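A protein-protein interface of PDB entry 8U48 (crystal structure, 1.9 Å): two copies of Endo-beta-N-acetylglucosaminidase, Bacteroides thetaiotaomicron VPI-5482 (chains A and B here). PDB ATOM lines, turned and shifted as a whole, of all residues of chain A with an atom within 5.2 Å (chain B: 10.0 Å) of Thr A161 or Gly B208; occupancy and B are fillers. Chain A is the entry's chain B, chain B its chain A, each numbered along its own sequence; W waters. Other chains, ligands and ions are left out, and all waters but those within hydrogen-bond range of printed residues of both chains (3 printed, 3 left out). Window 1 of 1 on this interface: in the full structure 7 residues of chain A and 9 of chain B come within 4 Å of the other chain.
ND2 of Asn A165 is in hydrogen-bond range of O of Gly B208.
OH of Tyr A189 is in hydrogen-bond range of O of Gly B208 (3.0 Å).
The side-chain hydroxyl (OH) of Tyr A189 is in hydrogen-bond range of the backbone carbonyl oxygen (O) of Met B209 (3.0 Å).
The side-chain hydroxyl (OH) of Tyr A189 sits close to the backbone nitrogen (N) of Pro B210 (3.4 Å).
The backbone carbonyl oxygen (O) of Thr B184 sits close to the side-chain amide nitrogen (ND2) of Asn B187 (3.4 Å).
The side-chain amide nitrogen of Asn B187 sits at hydrogen-bond distance from the backbone carbonyl oxygen of Phe B207 (3.2 Å).
ND2 of Asn B187 lies within hydrogen-bond range of O of Gly B208 (3.3 Å).
The backbone carbonyl oxygen of Asn B187 sits at hydrogen-bond distance from the side-chain amino group of Lys B213 (3.1 Å).
OG1 of Thr A161 is in hydrogen-bond range of O of Ser A157 (3.1 Å).
O of Thr A161 sits at hydrogen-bond distance from ND2 of Asn A165, at 3.1 Å.
Asn A158 touches Ser B188.
Asn B187 touches Thr A161.
O of Gly B208 touches CG2 of Thr A161, 3.6 Å away.
Thr B184 touches Asn A165.
Asn B187 touches Asn A165.
Ile A160 touches none of the printed residues of chain B.
Ala A162 touches none of the printed residues of chain B.
Printed residues of chain A within 4 Å of Ser B188: Asn A158 (3.6 Å).
Gly B208 touches just these residues of chain A: Thr A161, Asn A165 and Tyr A189.
Of the printed residues of chain A, Met B209 touches Tyr A189 (3.0 Å).
Of the printed residues of chain A, Pro B210 touches Tyr A189.
Phe B214 touches none of the printed residues of chain A.
The nearest residue of chain B that does not touch Thr A161 is Pro B210 (4.2 Å).
Hydrophobic or aromatic side chains of chain A that line the printed part of chain B: Tyr A189.
Of the 25 printed residues of chain B, 6 touch a printed residue of chain A.
Printed residues of chain B that touch a printed residue of chain A: Thr B184, Asn B187, Ser B188, Gly B208, Met B209 and Pro B210.
Among the printed residues, no Asp or Glu carboxylate lies within 4 Å of a Lys or Arg side-chain nitrogen of the other chain.
Positions printed for both chains: 186 and 189.
Of the 9 pairs that touch across the chains among the printed residues, none has its exchanged pair printed and touching as well.
Water W3 bridges NZ of Lys B213 and OD1 of Asn A158.
Water W2 lies within hydrogen-bond range of the backbone carbonyl oxygen (O) of Ser B188 (2.8 Å) and the side-chain amide nitrogen (ND2) of Asn A158 (3.0 Å).
Water W1 lies within hydrogen-bond range of the backbone carbonyl oxygen (O) of Met B209 (3.0 Å), the side-chain amide oxygen (OD1) of Asn B211 (3.0 Å), the side-chain hydroxyl (OH) of Tyr A189 (3.1 Å) and the side-chain hydroxyl (OG1) of Thr B205 (3.4 Å).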
ATOM      1  N   SER A 157      -8.994 -19.796  14.103  1.00  0.00           N
ATOM      2  CA  SER A 157      -9.803 -20.646  13.230  1.00  0.00           C
ATOM      3  C   SER A 157     -11.198 -20.862  13.798  1.00  0.00           C
ATOM      4  O   SER A 157     -12.182 -20.858  13.047  1.00  0.00           O
ATOM      5  CB  SER A 157      -9.108 -21.985  12.998  1.00  0.00           C
ATOM      6  OG  SER A 157      -7.913 -21.804  12.247  1.00  0.00           O
ATOM      7  N   ASN A 158     -11.307 -21.056  15.123  1.00  0.00           N
ATOM      8  CA  ASN A 158     -12.626 -21.216  15.729  1.00  0.00           C
ATOM      9  C   ASN A 158     -13.466 -19.955  15.601  1.00  0.00           C
ATOM     10  O   ASN A 158     -14.697 -20.041  15.481  1.00  0.00           O
ATOM     11  CB  ASN A 158     -12.496 -21.615  17.203  1.00  0.00           C
ATOM     12  CG  ASN A 158     -11.818 -22.958  17.378  1.00  0.00           C
ATOM     13  OD1 ASN A 158     -11.995 -23.855  16.559  1.00  0.00           O
ATOM     14  ND2 ASN A 158     -11.037 -23.106  18.445  1.00  0.00           N
ATOM     15  N   LEU A 159     -12.827 -18.779  15.648  1.00  0.00           N
ATOM     16  CA  LEU A 159     -13.567 -17.528  15.519  1.00  0.00           C
ATOM     17  C   LEU A 159     -14.209 -17.406  14.140  1.00  0.00           C
ATOM     18  O   LEU A 159     -15.365 -16.972  14.025  1.00  0.00           O
ATOM     19  CB  LEU A 159     -12.649 -16.337  15.802  1.00  0.00           C
ATOM     20  CG  LEU A 159     -13.261 -14.931  15.667  1.00  0.00           C
ATOM     21  CD1 LEU A 159     -14.527 -14.786  16.528  1.00  0.00           C
ATOM     22  CD2 LEU A 159     -12.242 -13.834  16.004  1.00  0.00           C
ATOM     23  N   ILE A 160     -13.478 -17.778  13.086  1.00  0.00           N
ATOM     24  CA  ILE A 160     -14.043 -17.777  11.735  1.00  0.00           C
ATOM     25  C   ILE A 160     -15.210 -18.753  11.646  1.00  0.00           C
ATOM     26  O   ILE A 160     -16.265 -18.446  11.076  1.00  0.00           O
ATOM     27  CB  ILE A 160     -12.962 -18.120  10.692  1.00  0.00           C
ATOM     28  CG1 ILE A 160     -11.784 -17.137  10.752  1.00  0.00           C
ATOM     29  CG2 ILE A 160     -13.560 -18.183   9.287  1.00  0.00           C
ATOM     30  CD1 ILE A 160     -12.149 -15.743  10.440  1.00  0.00           C
ATOM     31  N   THR A 161     -15.025 -19.953  12.192  1.00  0.00           N
ATOM     32  CA  THR A 161     -16.089 -20.955  12.187  1.00  0.00           C
ATOM     33  C   THR A 161     -17.323 -20.445  12.923  1.00  0.00           C
ATOM     34  O   THR A 161     -18.447 -20.518  12.406  1.00  0.00           O
ATOM     35  CB  THR A 161     -15.570 -22.246  12.826  1.00  0.00           C
ATOM     36  OG1 THR A 161     -14.463 -22.745  12.053  1.00  0.00           O
ATOM     37  CG2 THR A 161     -16.668 -23.308  12.904  1.00  0.00           C
ATOM     38  N   ALA A 162     -17.119 -19.915  14.134  1.00  0.00           N
ATOM     39  CA  ALA A 162     -18.230 -19.424  14.946  1.00  0.00           C
ATOM     40  C   ALA A 162     -18.966 -18.291  14.243  1.00  0.00           C
ATOM     41  O   ALA A 162     -20.199 -18.233  14.272  1.00  0.00           O
ATOM     42  CB  ALA A 162     -17.717 -18.965  16.314  1.00  0.00           C
ATOM     43  N   LEU A 163     -18.227 -17.394  13.581  1.00  0.00           N
ATOM     44  CA  LEU A 163     -18.864 -16.263  12.915  1.00  0.00           C
ATOM     45  C   LEU A 163     -19.609 -16.703  11.660  1.00  0.00           C
ATOM     46  O   LEU A 163     -20.748 -16.277  11.435  1.00  0.00           O
ATOM     47  CB  LEU A 163     -17.830 -15.187  12.584  1.00  0.00           C
ATOM     48  CG  LEU A 163     -18.378 -13.802  12.219  1.00  0.00           C
ATOM     49  CD1 LEU A 163     -19.432 -13.294  13.212  1.00  0.00           C
ATOM     50  CD2 LEU A 163     -17.242 -12.806  12.129  1.00  0.00           C
ATOM     51  N   HIS A 164     -18.991 -17.558  10.837  1.00  0.00           N
ATOM     52  CA  HIS A 164     -19.683 -18.103   9.671  1.00  0.00           C
ATOM     53  C   HIS A 164     -21.001 -18.753  10.064  1.00  0.00           C
ATOM     54  O   HIS A 164     -22.023 -18.571   9.393  1.00  0.00           O
ATOM     55  CB  HIS A 164     -18.805 -19.131   8.954  1.00  0.00           C
ATOM     56  CG  HIS A 164     -19.504 -19.841   7.833  1.00  0.00           C
ATOM     57  ND1 HIS A 164     -20.141 -21.054   7.996  1.00  0.00           N
ATOM     58  CD2 HIS A 164     -19.677 -19.500   6.533  1.00  0.00           C
ATOM     59  CE1 HIS A 164     -20.666 -21.435   6.844  1.00  0.00           C
ATOM     60  NE2 HIS A 164     -20.396 -20.510   5.938  1.00  0.00           N
ATOM     61  N   ASN A 165     -20.994 -19.517  11.153  1.00  0.00           N
ATOM     62  CA  ASN A 165     -22.213 -20.191  11.578  1.00  0.00           C
ATOM     63  C   ASN A 165     -23.257 -19.212  12.091  1.00  0.00           C
ATOM     64  O   ASN A 165     -24.454 -19.483  11.974  1.00  0.00           O
ATOM     65  CB  ASN A 165     -21.874 -21.236  12.636  1.00  0.00           C
ATOM     66  CG  ASN A 165     -21.158 -22.426  12.032  1.00  0.00           C
ATOM     67  OD1 ASN A 165     -21.443 -22.811  10.898  1.00  0.00           O
ATOM     68  ND2 ASN A 165     -20.214 -23.000  12.767  1.00  0.00           N
ATOM     69  N   LYS A 166     -22.834 -18.069  12.642  1.00  0.00           N
ATOM     70  CA  LYS A 166     -23.784 -17.101  13.187  1.00  0.00           C
ATOM     71  C   LYS A 166     -24.340 -16.135  12.148  1.00  0.00           C
ATOM     72  O   LYS A 166     -25.475 -15.658  12.304  1.00  0.00           O
ATOM     73  CB  LYS A 166     -23.137 -16.290  14.307  1.00  0.00           C
ATOM     74  CG  LYS A 166     -22.886 -17.087  15.583  1.00  0.00           C
ATOM     75  CD  LYS A 166     -22.160 -16.222  16.579  1.00  0.00           C
ATOM     76  CE  LYS A 166     -21.615 -17.060  17.724  1.00  0.00           C
ATOM     77  NZ  LYS A 166     -22.748 -17.627  18.508  1.00  0.00           N
ATOM     78  N   VAL A 186      -9.968 -23.695   7.805  1.00  0.00           N
ATOM     79  CA  VAL A 186     -11.271 -23.055   7.691  1.00  0.00           C
ATOM     80  C   VAL A 186     -11.375 -22.180   6.441  1.00  0.00           C
ATOM     81  O   VAL A 186     -12.245 -21.320   6.374  1.00  0.00           O
ATOM     82  CB  VAL A 186     -11.609 -22.239   8.952  1.00  0.00           C
ATOM     83  CG1 VAL A 186     -11.670 -23.142  10.187  1.00  0.00           C
ATOM     84  CG2 VAL A 186     -10.636 -21.065   9.128  1.00  0.00           C
ATOM     85  N   TYR A 189     -14.588 -21.154   4.540  1.00  0.00           N
ATOM     86  CA  TYR A 189     -15.422 -20.109   5.132  1.00  0.00           C
ATOM     87  C   TYR A 189     -14.925 -18.697   4.820  1.00  0.00           C
ATOM     88  O   TYR A 189     -15.555 -17.728   5.249  1.00  0.00           O
ATOM     89  CB  TYR A 189     -15.483 -20.268   6.660  1.00  0.00           C
ATOM     90  CG  TYR A 189     -16.223 -21.475   7.180  1.00  0.00           C
ATOM     91  CD1 TYR A 189     -17.184 -22.127   6.415  1.00  0.00           C
ATOM     92  CD2 TYR A 189     -15.973 -21.949   8.463  1.00  0.00           C
ATOM     93  CE1 TYR A 189     -17.864 -23.227   6.910  1.00  0.00           C
ATOM     94  CE2 TYR A 189     -16.649 -23.044   8.963  1.00  0.00           C
ATOM     95  CZ  TYR A 189     -17.587 -23.677   8.190  1.00  0.00           C
ATOM     96  OH  TYR A 189     -18.252 -24.762   8.714  1.00  0.00           O
ATOM     97  N   ASN B 176     -22.795 -38.175  12.896  1.00  0.00           N
ATOM     98  CA  ASN B 176     -23.759 -37.088  12.693  1.00  0.00           C
ATOM     99  C   ASN B 176     -25.192 -37.629  12.585  1.00  0.00           C
ATOM    100  O   ASN B 176     -25.819 -37.645  11.523  1.00  0.00           O
ATOM    101  CB  ASN B 176     -23.381 -36.269  11.465  1.00  0.00           C
ATOM    102  CG  ASN B 176     -24.262 -35.042  11.302  1.00  0.00           C
ATOM    103  OD1 ASN B 176     -24.722 -34.466  12.294  1.00  0.00           O
ATOM    104  ND2 ASN B 176     -24.506 -34.638  10.047  1.00  0.00           N
ATOM    105  N   THR B 180     -27.620 -33.931  16.920  1.00  0.00           N
ATOM    106  CA  THR B 180     -26.342 -33.251  16.689  1.00  0.00           C
ATOM    107  C   THR B 180     -26.502 -31.812  16.222  1.00  0.00           C
ATOM    108  O   THR B 180     -25.565 -31.030  16.390  1.00  0.00           O
ATOM    109  CB  THR B 180     -25.498 -34.017  15.662  1.00  0.00           C
ATOM    110  OG1 THR B 180     -26.206 -34.111  14.419  1.00  0.00           O
ATOM    111  CG2 THR B 180     -25.162 -35.411  16.171  1.00  0.00           C
ATOM    112  N   SER B 181     -27.645 -31.434  15.633  1.00  0.00           N
ATOM    113  CA  SER B 181     -27.804 -30.034  15.239  1.00  0.00           C
ATOM    114  C   SER B 181     -27.592 -29.083  16.417  1.00  0.00           C
ATOM    115  O   SER B 181     -27.246 -27.918  16.202  1.00  0.00           O
ATOM    116  CB  SER B 181     -29.187 -29.798  14.611  1.00  0.00           C
ATOM    117  OG  SER B 181     -30.211 -29.817  15.589  1.00  0.00           O
ATOM    118  N   GLU B 182     -27.737 -29.565  17.659  1.00  0.00           N
ATOM    119  CA  GLU B 182     -27.567 -28.722  18.839  1.00  0.00           C
ATOM    120  C   GLU B 182     -26.112 -28.408  19.162  1.00  0.00           C
ATOM    121  O   GLU B 182     -25.860 -27.549  20.015  1.00  0.00           O
ATOM    122  CB  GLU B 182     -28.183 -29.392  20.075  1.00  0.00           C
ATOM    123  CG  GLU B 182     -29.657 -29.699  19.980  1.00  0.00           C
ATOM    124  CD  GLU B 182     -30.190 -30.289  21.285  1.00  0.00           C
ATOM    125  OE1 GLU B 182     -29.367 -30.747  22.112  1.00  0.00           O
ATOM    126  OE2 GLU B 182     -31.415 -30.292  21.485  1.00  0.00           O
ATOM    127  N   LEU B 183     -25.160 -29.083  18.526  1.00  0.00           N
ATOM    128  CA  LEU B 183     -23.765 -29.062  18.941  1.00  0.00           C
ATOM    129  C   LEU B 183     -22.934 -27.960  18.290  1.00  0.00           C
ATOM    130  O   LEU B 183     -21.730 -27.895  18.549  1.00  0.00           O
ATOM    131  CB  LEU B 183     -23.111 -30.414  18.638  1.00  0.00           C
ATOM    132  CG  LEU B 183     -23.685 -31.611  19.396  1.00  0.00           C
ATOM    133  CD1 LEU B 183     -22.938 -32.886  19.006  1.00  0.00           C
ATOM    134  CD2 LEU B 183     -23.641 -31.369  20.916  1.00  0.00           C
ATOM    135  N   THR B 184     -23.533 -27.095  17.464  1.00  0.00           N
ATOM    136  CA  THR B 184     -22.734 -26.114  16.734  1.00  0.00           C
ATOM    137  C   THR B 184     -21.901 -25.252  17.683  1.00  0.00           C
ATOM    138  O   THR B 184     -20.721 -24.985  17.417  1.00  0.00           O
ATOM    139  CB  THR B 184     -23.645 -25.249  15.859  1.00  0.00           C
ATOM    140  OG1 THR B 184     -24.323 -26.088  14.914  1.00  0.00           O
ATOM    141  CG2 THR B 184     -22.830 -24.208  15.101  1.00  0.00           C
ATOM    142  N   GLY B 185     -22.482 -24.853  18.816  1.00  0.00           N
ATOM    143  CA  GLY B 185     -21.811 -23.972  19.754  1.00  0.00           C
ATOM    144  C   GLY B 185     -20.613 -24.589  20.451  1.00  0.00           C
ATOM    145  O   GLY B 185     -19.763 -23.848  20.953  1.00  0.00           O
ATOM    146  N   VAL B 186     -20.512 -25.915  20.479  1.00  0.00           N
ATOM    147  CA  VAL B 186     -19.378 -26.576  21.117  1.00  0.00           C
ATOM    148  C   VAL B 186     -18.516 -27.325  20.099  1.00  0.00           C
ATOM    149  O   VAL B 186     -17.741 -28.204  20.477  1.00  0.00           O
ATOM    150  CB  VAL B 186     -19.830 -27.517  22.250  1.00  0.00           C
ATOM    151  CG1 VAL B 186     -20.570 -26.747  23.357  1.00  0.00           C
ATOM    152  CG2 VAL B 186     -20.657 -28.694  21.703  1.00  0.00           C
ATOM    153  N   ASN B 187     -18.619 -26.994  18.809  1.00  0.00           N
ATOM    154  CA  ASN B 187     -17.912 -27.834  17.848  1.00  0.00           C
ATOM    155  C   ASN B 187     -16.394 -27.646  17.884  1.00  0.00           C
ATOM    156  O   ASN B 187     -15.687 -28.484  17.313  1.00  0.00           O
ATOM    157  CB  ASN B 187     -18.464 -27.637  16.418  1.00  0.00           C
ATOM    158  CG  ASN B 187     -18.087 -26.299  15.790  1.00  0.00           C
ATOM    159  OD1 ASN B 187     -17.139 -25.634  16.209  1.00  0.00           O
ATOM    160  ND2 ASN B 187     -18.826 -25.913  14.742  1.00  0.00           N
ATOM    161  N   SER B 188     -15.874 -26.592  18.531  1.00  0.00           N
ATOM    162  CA  SER B 188     -14.426 -26.486  18.686  1.00  0.00           C
ATOM    163  C   SER B 188     -13.850 -27.584  19.582  1.00  0.00           C
ATOM    164  O   SER B 188     -12.649 -27.867  19.492  1.00  0.00           O
ATOM    165  CB  SER B 188     -14.023 -25.110  19.236  1.00  0.00           C
ATOM    166  OG  SER B 188     -14.343 -24.956  20.613  1.00  0.00           O
ATOM    167  N   TYR B 189     -14.676 -28.211  20.425  1.00  0.00           N
ATOM    168  CA  TYR B 189     -14.300 -29.345  21.265  1.00  0.00           C
ATOM    169  C   TYR B 189     -14.396 -30.687  20.551  1.00  0.00           C
ATOM    170  O   TYR B 189     -14.060 -31.710  21.155  1.00  0.00           O
ATOM    171  CB  TYR B 189     -15.209 -29.427  22.499  1.00  0.00           C
ATOM    172  CG  TYR B 189     -15.273 -28.186  23.360  1.00  0.00           C
ATOM    173  CD1 TYR B 189     -14.187 -27.324  23.474  1.00  0.00           C
ATOM    174  CD2 TYR B 189     -16.426 -27.898  24.096  1.00  0.00           C
ATOM    175  CE1 TYR B 189     -14.258 -26.185  24.285  1.00  0.00           C
ATOM    176  CE2 TYR B 189     -16.505 -26.771  24.900  1.00  0.00           C
ATOM    177  CZ  TYR B 189     -15.426 -25.918  24.985  1.00  0.00           C
ATOM    178  OH  TYR B 189     -15.528 -24.806  25.787  1.00  0.00           O
ATOM    179  N   ILE B 190     -14.900 -30.720  19.323  1.00  0.00           N
ATOM    180  CA  ILE B 190     -15.122 -31.956  18.571  1.00  0.00           C
ATOM    181  C   ILE B 190     -14.068 -32.032  17.467  1.00  0.00           C
ATOM    182  O   ILE B 190     -13.957 -31.112  16.647  1.00  0.00           O
ATOM    183  CB  ILE B 190     -16.547 -31.996  17.988  1.00  0.00           C
ATOM    184  CG1 ILE B 190     -17.595 -31.867  19.099  1.00  0.00           C
ATOM    185  CG2 ILE B 190     -16.791 -33.284  17.182  1.00  0.00           C
ATOM    186  CD1 ILE B 190     -18.982 -31.445  18.577  1.00  0.00           C
ATOM    187  N   TYR B 192     -13.780 -34.537  14.969  1.00  0.00           N
ATOM    188  CA  TYR B 192     -14.335 -34.941  13.678  1.00  0.00           C
ATOM    189  C   TYR B 192     -15.827 -35.228  13.790  1.00  0.00           C
ATOM    190  O   TYR B 192     -16.302 -35.710  14.818  1.00  0.00           O
ATOM    191  CB  TYR B 192     -13.612 -36.182  13.105  1.00  0.00           C
ATOM    192  CG  TYR B 192     -12.204 -35.869  12.704  1.00  0.00           C
ATOM    193  CD1 TYR B 192     -11.942 -35.194  11.517  1.00  0.00           C
ATOM    194  CD2 TYR B 192     -11.137 -36.187  13.534  1.00  0.00           C
ATOM    195  CE1 TYR B 192     -10.666 -34.865  11.158  1.00  0.00           C
ATOM    196  CE2 TYR B 192      -9.847 -35.876  13.175  1.00  0.00           C
ATOM    197  CZ  TYR B 192      -9.616 -35.207  11.985  1.00  0.00           C
ATOM    198  OH  TYR B 192      -8.329 -34.870  11.609  1.00  0.00           O
ATOM    199  N   GLY B 193     -16.557 -34.900  12.726  1.00  0.00           N
ATOM    200  CA  GLY B 193     -17.926 -35.353  12.526  1.00  0.00           C
ATOM    201  C   GLY B 193     -17.987 -36.298  11.340  1.00  0.00           C
ATOM    202  O   GLY B 193     -17.183 -36.190  10.408  1.00  0.00           O
ATOM    203  N   SER B 204     -21.707 -31.848   2.415  1.00  0.00           N
ATOM    204  CA  SER B 204     -22.084 -30.884   3.443  1.00  0.00           C
ATOM    205  C   SER B 204     -21.431 -31.315   4.752  1.00  0.00           C
ATOM    206  O   SER B 204     -20.777 -32.361   4.826  1.00  0.00           O
ATOM    207  CB  SER B 204     -23.608 -30.798   3.585  1.00  0.00           C
ATOM    208  OG  SER B 204     -24.148 -32.082   3.866  1.00  0.00           O
ATOM    209  N   THR B 205     -21.598 -30.499   5.792  1.00  0.00           N
ATOM    210  CA  THR B 205     -21.202 -30.912   7.138  1.00  0.00           C
ATOM    211  C   THR B 205     -22.351 -30.672   8.113  1.00  0.00           C
ATOM    212  O   THR B 205     -23.259 -29.885   7.848  1.00  0.00           O
ATOM    213  CB  THR B 205     -19.954 -30.169   7.659  1.00  0.00           C
ATOM    214  OG1 THR B 205     -20.303 -28.823   8.008  1.00  0.00           O
ATOM    215  CG2 THR B 205     -18.794 -30.197   6.638  1.00  0.00           C
ATOM    216  N   GLY B 206     -22.281 -31.343   9.269  1.00  0.00           N
ATOM    217  CA  GLY B 206     -23.241 -31.147  10.331  1.00  0.00           C
ATOM    218  C   GLY B 206     -22.696 -30.260  11.434  1.00  0.00           C
ATOM    219  O   GLY B 206     -21.488 -30.064  11.555  1.00  0.00           O
ATOM    220  N   PHE B 207     -23.621 -29.762  12.258  1.00  0.00           N
ATOM    221  CA  PHE B 207     -23.358 -28.866  13.394  1.00  0.00           C
ATOM    222  C   PHE B 207     -22.219 -27.889  13.113  1.00  0.00           C
ATOM    223  O   PHE B 207     -21.340 -27.657  13.950  1.00  0.00           O
ATOM    224  CB  PHE B 207     -23.132 -29.651  14.710  1.00  0.00           C
ATOM    225  CG  PHE B 207     -22.248 -30.889  14.587  1.00  0.00           C
ATOM    226  CD1 PHE B 207     -22.739 -32.071  14.043  1.00  0.00           C
ATOM    227  CD2 PHE B 207     -20.953 -30.879  15.093  1.00  0.00           C
ATOM    228  CE1 PHE B 207     -21.931 -33.206  13.955  1.00  0.00           C
ATOM    229  CE2 PHE B 207     -20.143 -32.004  15.015  1.00  0.00           C
ATOM    230  CZ  PHE B 207     -20.632 -33.171  14.445  1.00  0.00           C
ATOM    231  N   GLY B 208     -22.256 -27.304  11.911  1.00  0.00           N
ATOM    232  CA  GLY B 208     -21.388 -26.195  11.555  1.00  0.00           C
ATOM    233  C   GLY B 208     -19.911 -26.517  11.443  1.00  0.00           C
ATOM    234  O   GLY B 208     -19.088 -25.596  11.465  1.00  0.00           O
ATOM    235  N   MET B 209     -19.550 -27.788  11.308  1.00  0.00           N
ATOM    236  CA  MET B 209     -18.138 -28.155  11.250  1.00  0.00           C
ATOM    237  C   MET B 209     -17.504 -27.686   9.943  1.00  0.00           C
ATOM    238  O   MET B 209     -18.129 -27.766   8.884  1.00  0.00           O
ATOM    239  CB  MET B 209     -17.975 -29.671  11.377  1.00  0.00           C
ATOM    240  CG  MET B 209     -18.391 -30.189  12.735  1.00  0.00           C
ATOM    241  SD  MET B 209     -17.107 -29.888  13.964  1.00  0.00           S
ATOM    242  CE  MET B 209     -16.280 -31.492  13.957  1.00  0.00           C
ATOM    243  N   PRO B 210     -16.271 -27.188   9.982  1.00  0.00           N
ATOM    244  CA  PRO B 210     -15.548 -26.922   8.732  1.00  0.00           C
ATOM    245  C   PRO B 210     -15.268 -28.219   7.987  1.00  0.00           C
ATOM    246  O   PRO B 210     -15.207 -29.306   8.565  1.00  0.00           O
ATOM    247  CB  PRO B 210     -14.245 -26.252   9.193  1.00  0.00           C
ATOM    248  CG  PRO B 210     -14.065 -26.676  10.602  1.00  0.00           C
ATOM    249  CD  PRO B 210     -15.456 -26.903  11.177  1.00  0.00           C
ATOM    250  N   ASN B 211     -15.094 -28.089   6.675  1.00  0.00           N
ATOM    251  CA  ASN B 211     -14.884 -29.274   5.848  1.00  0.00           C
ATOM    252  C   ASN B 211     -13.686 -30.086   6.324  1.00  0.00           C
ATOM    253  O   ASN B 211     -13.688 -31.314   6.213  1.00  0.00           O
ATOM    254  CB  ASN B 211     -14.697 -28.868   4.382  1.00  0.00           C
ATOM    255  CG  ASN B 211     -15.963 -28.298   3.773  1.00  0.00           C
ATOM    256  OD1 ASN B 211     -17.044 -28.386   4.366  1.00  0.00           O
ATOM    257  ND2 ASN B 211     -15.841 -27.729   2.583  1.00  0.00           N
ATOM    258  N   SER B 212     -12.664 -29.422   6.852  1.00  0.00           N
ATOM    259  CA  SER B 212     -11.445 -30.103   7.284  1.00  0.00           C
ATOM    260  C   SER B 212     -11.653 -30.970   8.524  1.00  0.00           C
ATOM    261  O   SER B 212     -10.746 -31.737   8.883  1.00  0.00           O
ATOM    262  CB  SER B 212     -10.360 -29.064   7.566  1.00  0.00           C
ATOM    263  OG  SER B 212     -10.770 -28.221   8.636  1.00  0.00           O
ATOM    264  N   LYS B 213     -12.801 -30.858   9.198  1.00  0.00           N
ATOM    265  CA  LYS B 213     -13.083 -31.662  10.387  1.00  0.00           C
ATOM    266  C   LYS B 213     -14.276 -32.589  10.178  1.00  0.00           C
ATOM    267  O   LYS B 213     -14.922 -32.997  11.146  1.00  0.00           O
ATOM    268  CB  LYS B 213     -13.312 -30.760  11.603  1.00  0.00           C
ATOM    269  CG  LYS B 213     -12.116 -29.828  11.894  1.00  0.00           C
ATOM    270  CD  LYS B 213     -12.415 -28.815  13.003  1.00  0.00           C
ATOM    271  CE  LYS B 213     -12.923 -29.497  14.240  1.00  0.00           C
ATOM    272  NZ  LYS B 213     -13.333 -28.539  15.321  1.00  0.00           N
ATOM    273  N   PHE B 214     -14.580 -32.940   8.934  1.00  0.00           N
ATOM    274  CA  PHE B 214     -15.768 -33.727   8.652  1.00  0.00           C
ATOM    275  C   PHE B 214     -15.488 -34.789   7.601  1.00  0.00           C
ATOM    276  O   PHE B 214     -14.722 -34.564   6.663  1.00  0.00           O
ATOM    277  CB  PHE B 214     -16.919 -32.831   8.176  1.00  0.00           C
ATOM    278  CG  PHE B 214     -18.260 -33.397   8.493  1.00  0.00           C
ATOM    279  CD1 PHE B 214     -18.806 -33.237   9.760  1.00  0.00           C
ATOM    280  CD2 PHE B 214     -18.957 -34.145   7.547  1.00  0.00           C
ATOM    281  CE1 PHE B 214     -20.049 -33.782  10.068  1.00  0.00           C
ATOM    282  CE2 PHE B 214     -20.193 -34.695   7.848  1.00  0.00           C
ATOM    283  CZ  PHE B 214     -20.738 -34.518   9.117  1.00  0.00           C
HETATM  284  O   HOH W   1     -18.571 -26.533   6.182  1.00  0.00           O
HETATM  285  O   HOH W   2     -10.549 -26.085  18.875  1.00  0.00           O
HETATM  286  O   HOH W   3     -11.540 -26.777  16.173  1.00  0.00           O
